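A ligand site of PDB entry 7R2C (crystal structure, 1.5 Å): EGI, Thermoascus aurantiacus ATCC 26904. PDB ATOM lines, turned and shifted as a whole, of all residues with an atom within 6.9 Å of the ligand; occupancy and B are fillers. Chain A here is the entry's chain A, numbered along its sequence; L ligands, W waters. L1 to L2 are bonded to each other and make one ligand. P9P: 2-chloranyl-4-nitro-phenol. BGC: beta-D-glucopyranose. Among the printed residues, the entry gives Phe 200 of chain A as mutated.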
ATOM      1  N   HIS A  93       8.835  20.378 -11.539  1.00  0.00           N
ATOM      2  CA  HIS A  93       9.620  20.020 -10.356  1.00  0.00           C
ATOM      3  C   HIS A  93      10.811  20.959 -10.199  1.00  0.00           C
ATOM      4  O   HIS A  93      11.970  20.561 -10.248  1.00  0.00           O
ATOM      5  CB  HIS A  93      10.067  18.574 -10.477  1.00  0.00           C
ATOM      6  CG  HIS A  93      10.147  17.836  -9.183  1.00  0.00           C
ATOM      7  ND1 HIS A  93       9.049  17.405  -8.488  1.00  0.00           N
ATOM      8  CD2 HIS A  93      11.232  17.429  -8.489  1.00  0.00           C
ATOM      9  CE1 HIS A  93       9.453  16.758  -7.401  1.00  0.00           C
ATOM     10  NE2 HIS A  93      10.783  16.772  -7.370  1.00  0.00           N
ATOM     11  N   TYR A  95      11.220  23.897  -7.775  1.00  0.00           N
ATOM     12  CA  TYR A  95      11.691  24.545  -6.557  1.00  0.00           C
ATOM     13  C   TYR A  95      11.617  26.066  -6.636  1.00  0.00           C
ATOM     14  O   TYR A  95      12.403  26.770  -6.001  1.00  0.00           O
ATOM     15  CB  TYR A  95      13.123  24.087  -6.234  1.00  0.00           C
ATOM     16  CG  TYR A  95      13.266  22.589  -6.134  1.00  0.00           C
ATOM     17  CD1 TYR A  95      12.904  21.927  -4.967  1.00  0.00           C
ATOM     18  CD2 TYR A  95      13.714  21.834  -7.194  1.00  0.00           C
ATOM     19  CE1 TYR A  95      13.020  20.569  -4.856  1.00  0.00           C
ATOM     20  CE2 TYR A  95      13.820  20.457  -7.104  1.00  0.00           C
ATOM     21  CZ  TYR A  95      13.470  19.829  -5.925  1.00  0.00           C
ATOM     22  OH  TYR A  95      13.585  18.456  -5.805  1.00  0.00           O
ATOM     23  N   ASN A 132       7.042  22.439  -7.607  1.00  0.00           N
ATOM     24  CA  ASN A 132       7.408  21.553  -6.509  1.00  0.00           C
ATOM     25  C   ASN A 132       8.317  22.289  -5.521  1.00  0.00           C
ATOM     26  O   ASN A 132       9.360  22.814  -5.917  1.00  0.00           O
ATOM     27  CB  ASN A 132       8.154  20.351  -7.077  1.00  0.00           C
ATOM     28  CG  ASN A 132       8.702  19.486  -5.990  1.00  0.00           C
ATOM     29  OD1 ASN A 132       7.931  18.790  -5.371  1.00  0.00           O
ATOM     30  ND2 ASN A 132      10.016  19.543  -5.745  1.00  0.00           N
ATOM     31  N   GLU A 133       7.919  22.359  -4.255  1.00  0.00           N
ATOM     32  CA  GLU A 133       8.816  22.691  -3.129  1.00  0.00           C
ATOM     33  C   GLU A 133       9.568  24.024  -3.306  1.00  0.00           C
ATOM     34  O   GLU A 133      10.801  24.074  -3.361  1.00  0.00           O
ATOM     35  CB  GLU A 133       9.788  21.536  -2.844  1.00  0.00           C
ATOM     36  CG  GLU A 133       9.079  20.281  -2.371  1.00  0.00           C
ATOM     37  CD  GLU A 133      10.004  19.229  -1.816  1.00  0.00           C
ATOM     38  OE1 GLU A 133      11.238  19.384  -1.933  1.00  0.00           O
ATOM     39  OE2 GLU A 133       9.486  18.219  -1.307  1.00  0.00           O
ATOM     40  N   HIS A 135      11.349  27.148  -1.881  1.00  0.00           N
ATOM     41  CA  HIS A 135      12.190  27.175  -0.688  1.00  0.00           C
ATOM     42  C   HIS A 135      13.173  28.334  -0.792  1.00  0.00           C
ATOM     43  O   HIS A 135      13.479  28.813  -1.882  1.00  0.00           O
ATOM     44  CB  HIS A 135      12.947  25.862  -0.493  1.00  0.00           C
ATOM     45  CG  HIS A 135      13.980  25.612  -1.542  1.00  0.00           C
ATOM     46  ND1 HIS A 135      15.293  25.986  -1.402  1.00  0.00           N
ATOM     47  CD2 HIS A 135      13.881  25.047  -2.779  1.00  0.00           C
ATOM     48  CE1 HIS A 135      15.968  25.655  -2.491  1.00  0.00           C
ATOM     49  NE2 HIS A 135      15.133  25.083  -3.337  1.00  0.00           N
ATOM     50  N   SER A 169       9.370  26.677   2.365  1.00  0.00           N
ATOM     51  CA  SER A 169       9.918  25.635   3.237  1.00  0.00           C
ATOM     52  C   SER A 169       9.686  24.236   2.669  1.00  0.00           C
ATOM     53  O   SER A 169       9.282  23.315   3.374  1.00  0.00           O
ATOM     54  CB  SER A 169       9.403  25.740   4.678  1.00  0.00           C
ATOM     55  OG  SER A 169      10.071  26.759   5.401  1.00  0.00           O
ATOM     56  N   TRP A 170       9.883  24.088   1.360  1.00  0.00           N
ATOM     57  CA  TRP A 170       9.757  22.787   0.697  1.00  0.00           C
ATOM     58  C   TRP A 170       8.340  22.249   0.856  1.00  0.00           C
ATOM     59  O   TRP A 170       8.125  21.034   0.853  1.00  0.00           O
ATOM     60  CB  TRP A 170      10.816  21.777   1.152  1.00  0.00           C
ATOM     61  CG  TRP A 170      12.205  22.355   1.287  1.00  0.00           C
ATOM     62  CD1 TRP A 170      12.727  22.989   2.373  1.00  0.00           C
ATOM     63  CD2 TRP A 170      13.254  22.320   0.305  1.00  0.00           C
ATOM     64  NE1 TRP A 170      14.022  23.359   2.142  1.00  0.00           N
ATOM     65  CE2 TRP A 170      14.378  22.951   0.880  1.00  0.00           C
ATOM     66  CE3 TRP A 170      13.355  21.807  -1.001  1.00  0.00           C
ATOM     67  CZ2 TRP A 170      15.588  23.104   0.191  1.00  0.00           C
ATOM     68  CZ3 TRP A 170      14.563  21.945  -1.681  1.00  0.00           C
ATOM     69  CH2 TRP A 170      15.661  22.593  -1.084  1.00  0.00           C
ATOM     70  N   GLY A 172       6.572  21.928   3.346  1.00  0.00           N
ATOM     71  CA  GLY A 172       6.477  20.949   4.413  1.00  0.00           C
ATOM     72  C   GLY A 172       5.219  21.132   5.240  1.00  0.00           C
ATOM     73  O   GLY A 172       4.825  22.249   5.585  1.00  0.00           O
ATOM     74  N   TRP A 174       4.970  20.127   8.374  1.00  0.00           N
ATOM     75  CA  TRP A 174       5.366  20.423   9.756  1.00  0.00           C
ATOM     76  C   TRP A 174       5.720  21.876  10.006  1.00  0.00           C
ATOM     77  O   TRP A 174       5.605  22.331  11.158  1.00  0.00           O
ATOM     78  CB  TRP A 174       6.494  19.488  10.216  1.00  0.00           C
ATOM     79  CG  TRP A 174       7.779  19.508   9.406  1.00  0.00           C
ATOM     80  CD1 TRP A 174       7.947  19.883   8.089  1.00  0.00           C
ATOM     81  CD2 TRP A 174       9.061  19.114   9.877  1.00  0.00           C
ATOM     82  NE1 TRP A 174       9.272  19.718   7.734  1.00  0.00           N
ATOM     83  CE2 TRP A 174       9.973  19.260   8.811  1.00  0.00           C
ATOM     84  CE3 TRP A 174       9.534  18.639  11.106  1.00  0.00           C
ATOM     85  CZ2 TRP A 174      11.331  18.951   8.946  1.00  0.00           C
ATOM     86  CZ3 TRP A 174      10.878  18.333  11.232  1.00  0.00           C
ATOM     87  CH2 TRP A 174      11.761  18.484  10.157  1.00  0.00           C
ATOM     88  N   THR A 175       6.121  22.614   8.975  1.00  0.00           N
ATOM     89  CA  THR A 175       6.449  24.023   9.112  1.00  0.00           C
ATOM     90  C   THR A 175       5.374  24.909   8.516  1.00  0.00           C
ATOM     91  O   THR A 175       5.554  26.139   8.491  1.00  0.00           O
ATOM     92  CB  THR A 175       7.789  24.304   8.442  1.00  0.00           C
ATOM     93  OG1 THR A 175       7.763  23.762   7.125  1.00  0.00           O
ATOM     94  CG2 THR A 175       8.908  23.654   9.226  1.00  0.00           C
ATOM     95  N   HIS A 198       4.146  18.396   1.718  1.00  0.00           N
ATOM     96  CA  HIS A 198       4.982  17.208   1.702  1.00  0.00           C
ATOM     97  C   HIS A 198       5.388  16.901   3.136  1.00  0.00           C
ATOM     98  O   HIS A 198       5.525  17.815   3.949  1.00  0.00           O
ATOM     99  CB  HIS A 198       6.252  17.406   0.855  1.00  0.00           C
ATOM    100  CG  HIS A 198       5.953  17.668  -0.594  1.00  0.00           C
ATOM    101  ND1 HIS A 198       6.939  17.976  -1.508  1.00  0.00           N
ATOM    102  CD2 HIS A 198       4.779  17.664  -1.269  1.00  0.00           C
ATOM    103  CE1 HIS A 198       6.385  18.167  -2.698  1.00  0.00           C
ATOM    104  NE2 HIS A 198       5.080  17.974  -2.583  1.00  0.00           N
ATOM    105  N   GLN A 199       5.587  15.624   3.423  1.00  0.00           N
ATOM    106  CA  GLN A 199       6.046  15.265   4.762  1.00  0.00           C
ATOM    107  C   GLN A 199       6.890  14.002   4.679  1.00  0.00           C
ATOM    108  O   GLN A 199       6.373  12.916   4.400  1.00  0.00           O
ATOM    109  CB  GLN A 199       4.889  15.039   5.725  1.00  0.00           C
ATOM    110  CG  GLN A 199       5.318  15.126   7.210  1.00  0.00           C
ATOM    111  CD  GLN A 199       6.087  16.393   7.489  1.00  0.00           C
ATOM    112  OE1 GLN A 199       5.491  17.464   7.573  1.00  0.00           O
ATOM    113  NE2 GLN A 199       7.402  16.298   7.652  1.00  0.00           N
ATOM    114  N   PHE A 200       8.165  14.159   5.003  1.00  0.00           N
ATOM    115  CA  PHE A 200       9.039  13.026   5.231  1.00  0.00           C
ATOM    116  C   PHE A 200       9.220  12.823   6.727  1.00  0.00           C
ATOM    117  O   PHE A 200       8.836  13.657   7.561  1.00  0.00           O
ATOM    118  CB  PHE A 200      10.335  13.236   4.455  1.00  0.00           C
ATOM    119  CG  PHE A 200      10.121  13.156   2.957  1.00  0.00           C
ATOM    120  CD1 PHE A 200      10.038  11.932   2.320  1.00  0.00           C
ATOM    121  CD2 PHE A 200       9.918  14.310   2.229  1.00  0.00           C
ATOM    122  CE1 PHE A 200       9.815  11.859   0.943  1.00  0.00           C
ATOM    123  CE2 PHE A 200       9.684  14.252   0.874  1.00  0.00           C
ATOM    124  CZ  PHE A 200       9.622  13.032   0.226  1.00  0.00           C
ATOM    125  N   ASP A 202      12.109  11.196   8.350  1.00  0.00           N
ATOM    126  CA  ASP A 202      13.431  11.067   8.941  1.00  0.00           C
ATOM    127  C   ASP A 202      13.740  12.270   9.825  1.00  0.00           C
ATOM    128  O   ASP A 202      12.960  13.221   9.902  1.00  0.00           O
ATOM    129  CB  ASP A 202      14.541  10.846   7.904  1.00  0.00           C
ATOM    130  CG  ASP A 202      14.475  11.783   6.705  1.00  0.00           C
ATOM    131  OD1 ASP A 202      13.532  12.612   6.574  1.00  0.00           O
ATOM    132  OD2 ASP A 202      15.470  11.776   5.947  1.00  0.00           O
ATOM    133  N   ASP A 204      15.556  14.976   9.871  1.00  0.00           N
ATOM    134  CA  ASP A 204      15.526  16.354   9.409  1.00  0.00           C
ATOM    135  C   ASP A 204      14.370  16.634   8.456  1.00  0.00           C
ATOM    136  O   ASP A 204      14.215  17.772   8.016  1.00  0.00           O
ATOM    137  CB  ASP A 204      16.884  16.776   8.830  1.00  0.00           C
ATOM    138  CG  ASP A 204      17.272  15.993   7.598  1.00  0.00           C
ATOM    139  OD1 ASP A 204      16.509  15.088   7.177  1.00  0.00           O
ATOM    140  OD2 ASP A 204      18.361  16.257   7.040  1.00  0.00           O
ATOM    141  N   GLY A 205      13.564  15.628   8.137  1.00  0.00           N
ATOM    142  CA  GLY A 205      12.468  15.839   7.208  1.00  0.00           C
ATOM    143  C   GLY A 205      12.873  15.976   5.767  1.00  0.00           C
ATOM    144  O   GLY A 205      12.070  16.425   4.933  1.00  0.00           O
ATOM    145  N   SER A 206      14.114  15.600   5.438  1.00  0.00           N
ATOM    146  CA  SER A 206      14.587  15.705   4.065  1.00  0.00           C
ATOM    147  C   SER A 206      14.206  14.496   3.222  1.00  0.00           C
ATOM    148  O   SER A 206      14.333  14.562   1.991  1.00  0.00           O
ATOM    149  CB  SER A 206      16.119  15.869   4.034  1.00  0.00           C
ATOM    150  OG  SER A 206      16.755  14.693   4.493  1.00  0.00           O
ATOM    151  N   GLY A 207      13.759  13.416   3.846  1.00  0.00           N
ATOM    152  CA  GLY A 207      13.460  12.209   3.082  1.00  0.00           C
ATOM    153  C   GLY A 207      14.685  11.616   2.435  1.00  0.00           C
ATOM    154  O   GLY A 207      14.601  11.128   1.294  1.00  0.00           O
ATOM    155  N   THR A 208      15.832  11.675   3.104  1.00  0.00           N
ATOM    156  CA  THR A 208      17.042  11.061   2.575  1.00  0.00           C
ATOM    157  C   THR A 208      17.509   9.845   3.355  1.00  0.00           C
ATOM    158  O   THR A 208      18.396   9.130   2.873  1.00  0.00           O
ATOM    159  CB  THR A 208      18.195  12.069   2.487  1.00  0.00           C
ATOM    160  OG1 THR A 208      18.402  12.668   3.776  1.00  0.00           O
ATOM    161  CG2 THR A 208      17.882  13.135   1.453  1.00  0.00           C
ATOM    162  N   GLU A 240       3.823  14.394  -1.363  1.00  0.00           N
ATOM    163  CA  GLU A 240       4.975  13.498  -1.271  1.00  0.00           C
ATOM    164  C   GLU A 240       5.069  13.075   0.189  1.00  0.00           C
ATOM    165  O   GLU A 240       4.984  13.934   1.081  1.00  0.00           O
ATOM    166  CB  GLU A 240       6.273  14.214  -1.625  1.00  0.00           C
ATOM    167  CG  GLU A 240       6.406  14.577  -3.083  1.00  0.00           C
ATOM    168  CD  GLU A 240       7.800  15.088  -3.405  1.00  0.00           C
ATOM    169  OE1 GLU A 240       8.753  14.779  -2.662  1.00  0.00           O
ATOM    170  OE2 GLU A 240       7.956  15.774  -4.437  1.00  0.00           O
HETATM  171 CL1  P9P L   1      16.952  19.493   6.064  1.00  0.00          CL
HETATM  172  C02 P9P L   1      15.279  20.072   5.895  1.00  0.00           C
HETATM  173  C03 P9P L   1      14.639  20.666   6.945  1.00  0.00           C
HETATM  174  C04 P9P L   1      13.343  21.097   6.778  1.00  0.00           C
HETATM  175  N05 P9P L   1      12.683  21.733   7.882  1.00  0.00           N
HETATM  176  O06 P9P L   1      11.596  22.161   7.762  1.00  0.00           O
HETATM  177  O07 P9P L   1      13.356  21.823   9.093  1.00  0.00           O
HETATM  178  C08 P9P L   1      12.675  20.948   5.573  1.00  0.00           C
HETATM  179  C09 P9P L   1      13.329  20.352   4.522  1.00  0.00           C
HETATM  180  C10 P9P L   1      14.631  19.913   4.688  1.00  0.00           C
HETATM  181  O11 P9P L   1      15.324  19.296   3.636  1.00  0.00           O
HETATM  182  C2  BGC L   2      15.863  18.915   1.340  1.00  0.00           C
HETATM  183  C3  BGC L   2      15.247  18.808  -0.044  1.00  0.00           C
HETATM  184  C4  BGC L   2      14.069  17.839  -0.042  1.00  0.00           C
HETATM  185  C5  BGC L   2      13.066  18.270   1.020  1.00  0.00           C
HETATM  186  C6  BGC L   2      11.921  17.299   1.172  1.00  0.00           C
HETATM  187  C1  BGC L   2      14.790  19.274   2.368  1.00  0.00           C
HETATM  188  O2  BGC L   2      16.861  19.926   1.365  1.00  0.00           O
HETATM  189  O3  BGC L   2      16.216  18.366  -0.976  1.00  0.00           O
HETATM  190  O4  BGC L   2      13.415  17.830  -1.307  1.00  0.00           O
HETATM  191  O5  BGC L   2      13.716  18.337   2.300  1.00  0.00           O
HETATM  192  O6  BGC L   2      11.223  17.553   2.386  1.00  0.00           O
HETATM  193  O   HOH W   1      13.828  20.758  12.192  1.00  0.00           O
HETATM  194  O   HOH W   2      17.130  22.148   3.764  1.00  0.00           O
HETATM  195  O   HOH W   3       8.906  19.034   2.830  1.00  0.00           O
HETATM  196  O   HOH W   4      16.576  15.270  -1.147  1.00  0.00           O
HETATM  197  O   HOH W   5       9.654  20.633   5.002  1.00  0.00           O
HETATM  198  O   HOH W   6      15.289  19.733  10.011  1.00  0.00           O
HETATM  199  O   HOH W   7       9.308  16.884   5.232  1.00  0.00           O
HETATM  200  O   HOH W   8      18.246  20.088  -1.322  1.00  0.00           O
HETATM  201  O   HOH W   9      15.834  18.727  -3.641  1.00  0.00           O
HETATM  202  O   HOH W  10      11.335  21.923  11.048  1.00  0.00           O
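The side-chain carboxylate (OE1) of Glu 133 lies within hydrogen-bond range of an oxygen (O4) of BGC L2, at 2.7 Å.
The backbone carbonyl oxygen (O) of Gly 205 sits at hydrogen-bond distance from an oxygen (O6) of BGC L2 (2.9 Å).
An oxygen (O06) of P9P L1 sits at hydrogen-bond distance from the indole nitrogen (NE1) of Trp 174 (3.4 Å).
The side-chain carboxylate of Glu 133 is in hydrogen-bond range of a ring nitrogen (ND1) of His 198.
The backbone NH (N) of Gly 205 lies within hydrogen-bond range of the side-chain carboxylate (OD1) of Asp 202 (3.4 Å).
OD1 of Asp 204 is in hydrogen-bond range of OG of Ser 206.
The backbone NH (N) of Trp 174 lies within hydrogen-bond range of the side-chain amide oxygen (OE1) of Gln 199, 2.8 Å away.
The side-chain hydroxyl (OG) of Ser 206 sits at hydrogen-bond distance from the side-chain hydroxyl (OG1) of Thr 208, 2.7 Å away.
N of Ser 206 sits at hydrogen-bond distance from OD1 of Asp 202 (3.2 Å).
Residues that only touch the ligand: Trp 170, Thr 175, Phe 200, Asp 204 and Ser 206.
Hydrophobic or aromatic side chains within 4 Å of the ligand: Trp 170, Trp 174 and Phe 200.
The nearest printed residue that does not touch the ligand is Tyr 95 (4.5 Å).
Water W9 bridges an oxygen (O3) of BGC L2 and the side-chain hydroxyl of Tyr 95.
Water W3 bridges O6 of BGC L2 and O of Trp 170.
Water W6 lies within hydrogen-bond range of an oxygen (O07) of P9P L1 (3.0 Å) and the backbone carbonyl oxygen of Asp 204 (3.0 Å).
Water W5 bridges NE1 of Trp 174 (2.9 Å) and O of Ser 169 (3.2 Å).
Water W7 lies within hydrogen-bond range of the backbone carbonyl oxygen of Gly 205, the backbone NH of Phe 200, the side-chain amide nitrogen of Gln 199 and an oxygen (O6) of BGC L2.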
